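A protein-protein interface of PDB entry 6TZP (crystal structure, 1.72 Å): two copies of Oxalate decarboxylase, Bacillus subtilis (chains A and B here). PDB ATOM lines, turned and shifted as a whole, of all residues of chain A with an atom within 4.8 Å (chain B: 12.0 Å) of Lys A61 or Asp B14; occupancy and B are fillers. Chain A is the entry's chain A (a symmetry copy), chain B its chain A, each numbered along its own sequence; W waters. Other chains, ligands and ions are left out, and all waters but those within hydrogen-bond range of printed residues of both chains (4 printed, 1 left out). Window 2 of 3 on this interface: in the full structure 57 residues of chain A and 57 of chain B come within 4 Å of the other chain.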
ATOM      1  N   LEU A  59     -21.832   3.756  -5.221  1.00  0.00           N
ATOM      2  CA  LEU A  59     -22.341   4.516  -6.364  1.00  0.00           C
ATOM      3  C   LEU A  59     -22.920   3.563  -7.409  1.00  0.00           C
ATOM      4  O   LEU A  59     -22.275   2.579  -7.787  1.00  0.00           O
ATOM      5  CB  LEU A  59     -21.229   5.370  -6.992  1.00  0.00           C
ATOM      6  CG  LEU A  59     -20.370   6.224  -6.045  1.00  0.00           C
ATOM      7  CD1 LEU A  59     -19.405   7.135  -6.821  1.00  0.00           C
ATOM      8  CD2 LEU A  59     -21.234   7.043  -5.073  1.00  0.00           C
ATOM      9  N   GLU A  60     -24.132   3.858  -7.880  1.00  0.00           N
ATOM     10  CA  GLU A  60     -24.774   3.073  -8.929  1.00  0.00           C
ATOM     11  C   GLU A  60     -25.332   4.014  -9.983  1.00  0.00           C
ATOM     12  O   GLU A  60     -25.478   5.218  -9.753  1.00  0.00           O
ATOM     13  CB  GLU A  60     -25.911   2.192  -8.375  1.00  0.00           C
ATOM     14  CG  GLU A  60     -25.476   1.186  -7.309  1.00  0.00           C
ATOM     15  CD  GLU A  60     -24.613   0.060  -7.871  1.00  0.00           C
ATOM     16  OE1 GLU A  60     -24.518  -0.083  -9.110  1.00  0.00           O
ATOM     17  OE2 GLU A  60     -24.018  -0.688  -7.068  1.00  0.00           O
ATOM     18  N   LYS A  61     -25.675   3.449 -11.145  1.00  0.00           N
ATOM     19  CA  LYS A  61     -26.431   4.213 -12.136  1.00  0.00           C
ATOM     20  C   LYS A  61     -27.809   4.478 -11.555  1.00  0.00           C
ATOM     21  O   LYS A  61     -28.621   3.554 -11.434  1.00  0.00           O
ATOM     22  CB  LYS A  61     -26.535   3.453 -13.457  1.00  0.00           C
ATOM     23  CG  LYS A  61     -25.196   3.101 -14.099  1.00  0.00           C
ATOM     24  CD  LYS A  61     -25.412   2.468 -15.476  1.00  0.00           C
ATOM     25  CE  LYS A  61     -24.095   2.032 -16.109  1.00  0.00           C
ATOM     26  NZ  LYS A  61     -24.284   1.665 -17.548  1.00  0.00           N
ATOM     27  N   GLY A  62     -28.066   5.726 -11.171  1.00  0.00           N
ATOM     28  CA  GLY A  62     -29.307   6.088 -10.511  1.00  0.00           C
ATOM     29  C   GLY A  62     -29.179   6.639  -9.105  1.00  0.00           C
ATOM     30  O   GLY A  62     -30.180   7.152  -8.576  1.00  0.00           O
ATOM     31  N   GLY A  63     -28.028   6.554  -8.440  1.00  0.00           N
ATOM     32  CA  GLY A  63     -27.943   7.133  -7.109  1.00  0.00           C
ATOM     33  C   GLY A  63     -26.782   6.553  -6.314  1.00  0.00           C
ATOM     34  O   GLY A  63     -25.796   6.085  -6.885  1.00  0.00           O
ATOM     35  N   ILE A 201     -30.036  -0.535  -7.460  1.00  0.00           N
ATOM     36  CA  ILE A 201     -30.538   0.785  -7.855  1.00  0.00           C
ATOM     37  C   ILE A 201     -30.369   0.895  -9.367  1.00  0.00           C
ATOM     38  O   ILE A 201     -29.293   0.578  -9.886  1.00  0.00           O
ATOM     39  CB  ILE A 201     -29.776   1.930  -7.154  1.00  0.00           C
ATOM     40  CG1 ILE A 201     -30.149   2.024  -5.669  1.00  0.00           C
ATOM     41  CG2 ILE A 201     -30.014   3.277  -7.857  1.00  0.00           C
ATOM     42  CD1 ILE A 201     -29.283   3.038  -4.882  1.00  0.00           C
ATOM     43  N   PHE A 202     -31.421   1.322 -10.078  1.00  0.00           N
ATOM     44  CA  PHE A 202     -31.298   1.442 -11.534  1.00  0.00           C
ATOM     45  C   PHE A 202     -32.117   2.611 -12.076  1.00  0.00           C
ATOM     46  O   PHE A 202     -33.156   2.977 -11.523  1.00  0.00           O
ATOM     47  CB  PHE A 202     -31.683   0.132 -12.265  1.00  0.00           C
ATOM     48  CG  PHE A 202     -33.073  -0.406 -11.954  1.00  0.00           C
ATOM     49  CD1 PHE A 202     -33.336  -1.061 -10.758  1.00  0.00           C
ATOM     50  CD2 PHE A 202     -34.086  -0.326 -12.900  1.00  0.00           C
ATOM     51  CE1 PHE A 202     -34.599  -1.582 -10.493  1.00  0.00           C
ATOM     52  CE2 PHE A 202     -35.353  -0.847 -12.640  1.00  0.00           C
ATOM     53  CZ  PHE A 202     -35.601  -1.476 -11.429  1.00  0.00           C
ATOM     54  N   GLU A 203     -31.623   3.203 -13.167  1.00  0.00           N
ATOM     55  CA  GLU A 203     -32.320   4.312 -13.809  1.00  0.00           C
ATOM     56  C   GLU A 203     -33.608   3.825 -14.458  1.00  0.00           C
ATOM     57  O   GLU A 203     -33.693   2.697 -14.958  1.00  0.00           O
ATOM     58  CB  GLU A 203     -31.434   4.974 -14.878  1.00  0.00           C
ATOM     59  CG  GLU A 203     -30.036   5.368 -14.410  1.00  0.00           C
ATOM     60  CD  GLU A 203     -29.930   6.807 -13.923  1.00  0.00           C
ATOM     61  OE1 GLU A 203     -30.936   7.349 -13.412  1.00  0.00           O
ATOM     62  OE2 GLU A 203     -28.827   7.395 -14.042  1.00  0.00           O
ATOM     63  N   GLN B   9     -18.239  15.769  -5.517  1.00  0.00           N
ATOM     64  CA  GLN B   9     -19.522  15.087  -5.588  1.00  0.00           C
ATOM     65  C   GLN B   9     -19.311  13.591  -5.742  1.00  0.00           C
ATOM     66  O   GLN B   9     -18.336  13.153  -6.371  1.00  0.00           O
ATOM     67  CB  GLN B   9     -20.371  15.593  -6.765  1.00  0.00           C
ATOM     68  CG  GLN B   9     -20.740  17.079  -6.679  1.00  0.00           C
ATOM     69  CD  GLN B   9     -21.775  17.383  -5.602  1.00  0.00           C
ATOM     70  OE1 GLN B   9     -22.286  16.482  -4.935  1.00  0.00           O
ATOM     71  NE2 GLN B   9     -22.106  18.667  -5.446  1.00  0.00           N
ATOM     72  N   PRO B  10     -20.221  12.786  -5.197  1.00  0.00           N
ATOM     73  CA  PRO B  10     -20.102  11.317  -5.303  1.00  0.00           C
ATOM     74  C   PRO B  10     -20.617  10.827  -6.650  1.00  0.00           C
ATOM     75  O   PRO B  10     -21.673  10.215  -6.777  1.00  0.00           O
ATOM     76  CB  PRO B  10     -20.934  10.830  -4.110  1.00  0.00           C
ATOM     77  CG  PRO B  10     -21.950  11.893  -3.889  1.00  0.00           C
ATOM     78  CD  PRO B  10     -21.302  13.199  -4.281  1.00  0.00           C
ATOM     79  N   ILE B  11     -19.837  11.132  -7.688  1.00  0.00           N
ATOM     80  CA  ILE B  11     -20.148  10.802  -9.072  1.00  0.00           C
ATOM     81  C   ILE B  11     -18.913  10.147  -9.676  1.00  0.00           C
ATOM     82  O   ILE B  11     -17.798  10.660  -9.522  1.00  0.00           O
ATOM     83  CB  ILE B  11     -20.547  12.051  -9.886  1.00  0.00           C
ATOM     84  CG1 ILE B  11     -21.869  12.631  -9.376  1.00  0.00           C
ATOM     85  CG2 ILE B  11     -20.645  11.707 -11.380  1.00  0.00           C
ATOM     86  CD1 ILE B  11     -22.189  14.028  -9.927  1.00  0.00           C
ATOM     87  N   ARG B  12     -19.109   9.008 -10.340  1.00  0.00           N
ATOM     88  CA  ARG B  12     -18.026   8.278 -11.006  1.00  0.00           C
ATOM     89  C   ARG B  12     -18.573   7.876 -12.373  1.00  0.00           C
ATOM     90  O   ARG B  12     -19.321   6.901 -12.482  1.00  0.00           O
ATOM     91  CB  ARG B  12     -17.588   7.062 -10.185  1.00  0.00           C
ATOM     92  CG  ARG B  12     -16.334   6.328 -10.688  1.00  0.00           C
ATOM     93  CD  ARG B  12     -15.950   5.158  -9.746  1.00  0.00           C
ATOM     94  NE  ARG B  12     -16.950   4.096  -9.766  1.00  0.00           N
ATOM     95  CZ  ARG B  12     -17.576   3.601  -8.700  1.00  0.00           C
ATOM     96  NH1 ARG B  12     -17.310   4.040  -7.467  1.00  0.00           N
ATOM     97  NH2 ARG B  12     -18.477   2.645  -8.873  1.00  0.00           N
ATOM     98  N   GLY B  13     -18.229   8.639 -13.400  1.00  0.00           N
ATOM     99  CA  GLY B  13     -18.762   8.349 -14.724  1.00  0.00           C
ATOM    100  C   GLY B  13     -20.264   8.531 -14.733  1.00  0.00           C
ATOM    101  O   GLY B  13     -20.783   9.600 -14.384  1.00  0.00           O
ATOM    102  N   ASP B  14     -20.990   7.481 -15.121  1.00  0.00           N
ATOM    103  CA  ASP B  14     -22.445   7.532 -15.132  1.00  0.00           C
ATOM    104  C   ASP B  14     -23.069   6.980 -13.850  1.00  0.00           C
ATOM    105  O   ASP B  14     -24.280   6.739 -13.820  1.00  0.00           O
ATOM    106  CB  ASP B  14     -22.998   6.799 -16.366  1.00  0.00           C
ATOM    107  CG  ASP B  14     -22.547   5.349 -16.458  1.00  0.00           C
ATOM    108  OD1 ASP B  14     -21.941   4.833 -15.494  1.00  0.00           O
ATOM    109  OD2 ASP B  14     -22.798   4.719 -17.515  1.00  0.00           O
ATOM    110  N   LYS B  15     -22.280   6.806 -12.789  1.00  0.00           N
ATOM    111  CA  LYS B  15     -22.766   6.319 -11.502  1.00  0.00           C
ATOM    112  C   LYS B  15     -22.710   7.424 -10.456  1.00  0.00           C
ATOM    113  O   LYS B  15     -21.875   8.329 -10.533  1.00  0.00           O
ATOM    114  CB  LYS B  15     -21.951   5.115 -11.023  1.00  0.00           C
ATOM    115  CG  LYS B  15     -22.109   3.890 -11.934  1.00  0.00           C
ATOM    116  CD  LYS B  15     -21.320   2.691 -11.429  1.00  0.00           C
ATOM    117  CE  LYS B  15     -21.399   1.556 -12.455  1.00  0.00           C
ATOM    118  NZ  LYS B  15     -20.617   0.359 -12.045  1.00  0.00           N
ATOM    119  N   GLY B  16     -23.613   7.341  -9.476  1.00  0.00           N
ATOM    120  CA  GLY B  16     -23.682   8.344  -8.423  1.00  0.00           C
ATOM    121  C   GLY B  16     -24.523   9.553  -8.801  1.00  0.00           C
ATOM    122  O   GLY B  16     -25.202   9.591  -9.832  1.00  0.00           O
ATOM    123  N   ALA B  17     -24.450  10.576  -7.947  1.00  0.00           N
ATOM    124  CA  ALA B  17     -25.292  11.765  -8.087  1.00  0.00           C
ATOM    125  C   ALA B  17     -24.759  12.855  -7.163  1.00  0.00           C
ATOM    126  O   ALA B  17     -23.944  12.589  -6.276  1.00  0.00           O
ATOM    127  CB  ALA B  17     -26.751  11.448  -7.751  1.00  0.00           C
ATOM    128  N   THR B  18     -25.234  14.090  -7.370  1.00  0.00           N
ATOM    129  CA  THR B  18     -24.872  15.166  -6.446  1.00  0.00           C
ATOM    130  C   THR B  18     -25.537  14.954  -5.085  1.00  0.00           C
ATOM    131  O   THR B  18     -26.600  14.330  -4.977  1.00  0.00           O
ATOM    132  CB  THR B  18     -25.280  16.532  -6.999  1.00  0.00           C
ATOM    133  OG1 THR B  18     -26.676  16.512  -7.313  1.00  0.00           O
ATOM    134  CG2 THR B  18     -24.478  16.873  -8.256  1.00  0.00           C
ATOM    135  N   LEU B  35     -15.943   9.098  -0.636  1.00  0.00           N
ATOM    136  CA  LEU B  35     -17.025   9.725  -1.401  1.00  0.00           C
ATOM    137  C   LEU B  35     -17.114   9.146  -2.811  1.00  0.00           C
ATOM    138  O   LEU B  35     -18.216   8.932  -3.341  1.00  0.00           O
ATOM    139  CB  LEU B  35     -16.804  11.234  -1.461  1.00  0.00           C
ATOM    140  CG  LEU B  35     -17.972  12.057  -2.016  1.00  0.00           C
ATOM    141  CD1 LEU B  35     -19.077  12.141  -0.972  1.00  0.00           C
ATOM    142  CD2 LEU B  35     -17.501  13.450  -2.418  1.00  0.00           C
ATOM    143  N   VAL B  36     -15.966   8.897  -3.439  1.00  0.00           N
ATOM    144  CA  VAL B  36     -15.921   8.280  -4.767  1.00  0.00           C
ATOM    145  C   VAL B  36     -14.952   7.102  -4.719  1.00  0.00           C
ATOM    146  O   VAL B  36     -13.772   7.248  -5.077  1.00  0.00           O
ATOM    147  CB  VAL B  36     -15.522   9.287  -5.861  1.00  0.00           C
ATOM    148  CG1 VAL B  36     -15.558   8.608  -7.233  1.00  0.00           C
ATOM    149  CG2 VAL B  36     -16.463  10.505  -5.850  1.00  0.00           C
ATOM    150  N   PRO B  37     -15.406   5.932  -4.283  1.00  0.00           N
ATOM    151  CA  PRO B  37     -14.521   4.770  -4.173  1.00  0.00           C
ATOM    152  C   PRO B  37     -14.107   4.254  -5.536  1.00  0.00           C
ATOM    153  O   PRO B  37     -14.739   4.564  -6.559  1.00  0.00           O
ATOM    154  CB  PRO B  37     -15.392   3.733  -3.443  1.00  0.00           C
ATOM    155  CG  PRO B  37     -16.416   4.559  -2.710  1.00  0.00           C
ATOM    156  CD  PRO B  37     -16.717   5.681  -3.661  1.00  0.00           C
ATOM    157  N   PRO B  38     -13.044   3.456  -5.579  1.00  0.00           N
ATOM    158  CA  PRO B  38     -12.700   2.740  -6.809  1.00  0.00           C
ATOM    159  C   PRO B  38     -13.845   1.833  -7.228  1.00  0.00           C
ATOM    160  O   PRO B  38     -14.576   1.294  -6.390  1.00  0.00           O
ATOM    161  CB  PRO B  38     -11.456   1.927  -6.413  1.00  0.00           C
ATOM    162  CG  PRO B  38     -10.915   2.618  -5.186  1.00  0.00           C
ATOM    163  CD  PRO B  38     -12.100   3.193  -4.478  1.00  0.00           C
ATOM    164  N   GLU B  39     -14.012   1.677  -8.543  1.00  0.00           N
ATOM    165  CA  GLU B  39     -15.047   0.768  -9.020  1.00  0.00           C
ATOM    166  C   GLU B  39     -14.759  -0.675  -8.638  1.00  0.00           C
ATOM    167  O   GLU B  39     -15.662  -1.513  -8.720  1.00  0.00           O
ATOM    168  CB  GLU B  39     -15.213   0.887 -10.541  1.00  0.00           C
ATOM    169  CG  GLU B  39     -14.061   0.332 -11.349  1.00  0.00           C
ATOM    170  CD  GLU B  39     -14.326   0.406 -12.847  1.00  0.00           C
ATOM    171  OE1 GLU B  39     -15.497   0.612 -13.233  1.00  0.00           O
ATOM    172  OE2 GLU B  39     -13.365   0.266 -13.634  1.00  0.00           O
HETATM  173  O   HOH W   1     -25.586   4.075 -18.971  1.00  0.00           O
HETATM  174  O   HOH W   2     -18.915   3.018  -5.021  1.00  0.00           O
HETATM  175  O   HOH W   3     -26.646   6.673 -15.317  1.00  0.00           O
HETATM  176  O   HOH W   4     -20.099   1.058  -7.462  1.00  0.00           O
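NZ of Lys A61 lies within salt-bridge range of OD2 of Asp B14 (3.4 Å).
N of Gly B16 lies within hydrogen-bond range of O of Glu A60 (2.8 Å).
The guanidinium group (NH1) of Arg B12 lies within hydrogen-bond range of the backbone carbonyl oxygen (O) of Pro B37, at 2.8 Å.
The backbone carbonyl oxygen (O) of Lys A61 lies within hydrogen-bond range of the backbone NH (N) of Glu A203, at 3.5 Å.
The backbone carbonyl oxygen (O) of Pro B10 is in hydrogen-bond range of the backbone NH (N) of Ala B17 (3.0 Å).
Leu A59 touches Pro B10.
Leu A59 touches Arg B12 (CD1 to NH1, 3.8 Å).
O of Leu A59 touches CD of Lys B15, 3.8 Å away.
Gly B16 touches Leu A59 (N to CB, 3.97 Å).
Leu B35 touches Leu A59 (O to CD2, 3.96 Å).
Glu A60 touches Lys B15 (O to CA, 3.4 Å).
Lys A61 touches Lys B15 (N to CG, 3.7 Å).
CA of Gly B16 touches O of Gly A63, 3.5 Å away.
Printed residues of chain B within 4 Å of Leu A59: Pro B10, Arg B12, Lys B15, Gly B16 and Leu B35.
Glu A60 touches just these residues of chain B: Lys B15 and Gly B16.
Of chain B, only Asp B14 (3.3 Å) and Lys B15 (3.7 Å) come within 4 Å of Lys A61.
Of chain B, only Gly B16 comes within 4 Å of Gly A63.
No residue of chain B comes within 4 Å of Ile A201.
Ile B11 touches none of the printed residues of chain A.
Of chain A, only Lys A61 comes within 4 Å of Asp B14.
Of the printed residues of chain A, Lys B15 touches Leu A59 (3.8 Å), Glu A60 (3.4 Å) and Lys A61 (3.7 Å).
Printed residues of chain A within 4 Å of Leu B35: Leu A59 (3.96 Å).
Val B36 touches none of the printed residues of chain A.
The nearest printed residue of chain A that does not touch Pro B10 is Gly A63 (5.8 Å).
Of the 8 printed residues of chain A, 4 touch a printed residue of chain B.
Hydrophobic or aromatic side chains of chain A that line the printed part of chain B: Leu A59.
Hydrophobic or aromatic side chains of chain B within 4 Å of the printed part of chain A: Pro B10.
Among the printed residues, 10 pairs touch across the chains.
Among the printed residues, Asp or Glu carboxylates within 4 Å of a Lys or Arg side-chain nitrogen of the other chain: Lys A61 with Asp B14 (3.4 Å).
No position is printed for both chains.
Of the 10 pairs that touch across the chains among the printed residues, none has its exchanged pair printed and touching as well.
Water W3 lies within hydrogen-bond range of the side-chain carboxylate of Glu A203 (2.6 Å) and the backbone carbonyl oxygen of Asp B14 (2.8 Å).
Water W4 lies within hydrogen-bond range of NH2 of Arg B12 (2.7 Å) and O of Leu A59 (2.7 Å).
Water W2 bridges N of Leu A59 (3.0 Å) and NH1 of Arg B12 (3.1 Å).
Water W1 bridges NZ of Lys A61 (3.1 Å) and OD2 of Asp B14 (3.2 Å).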
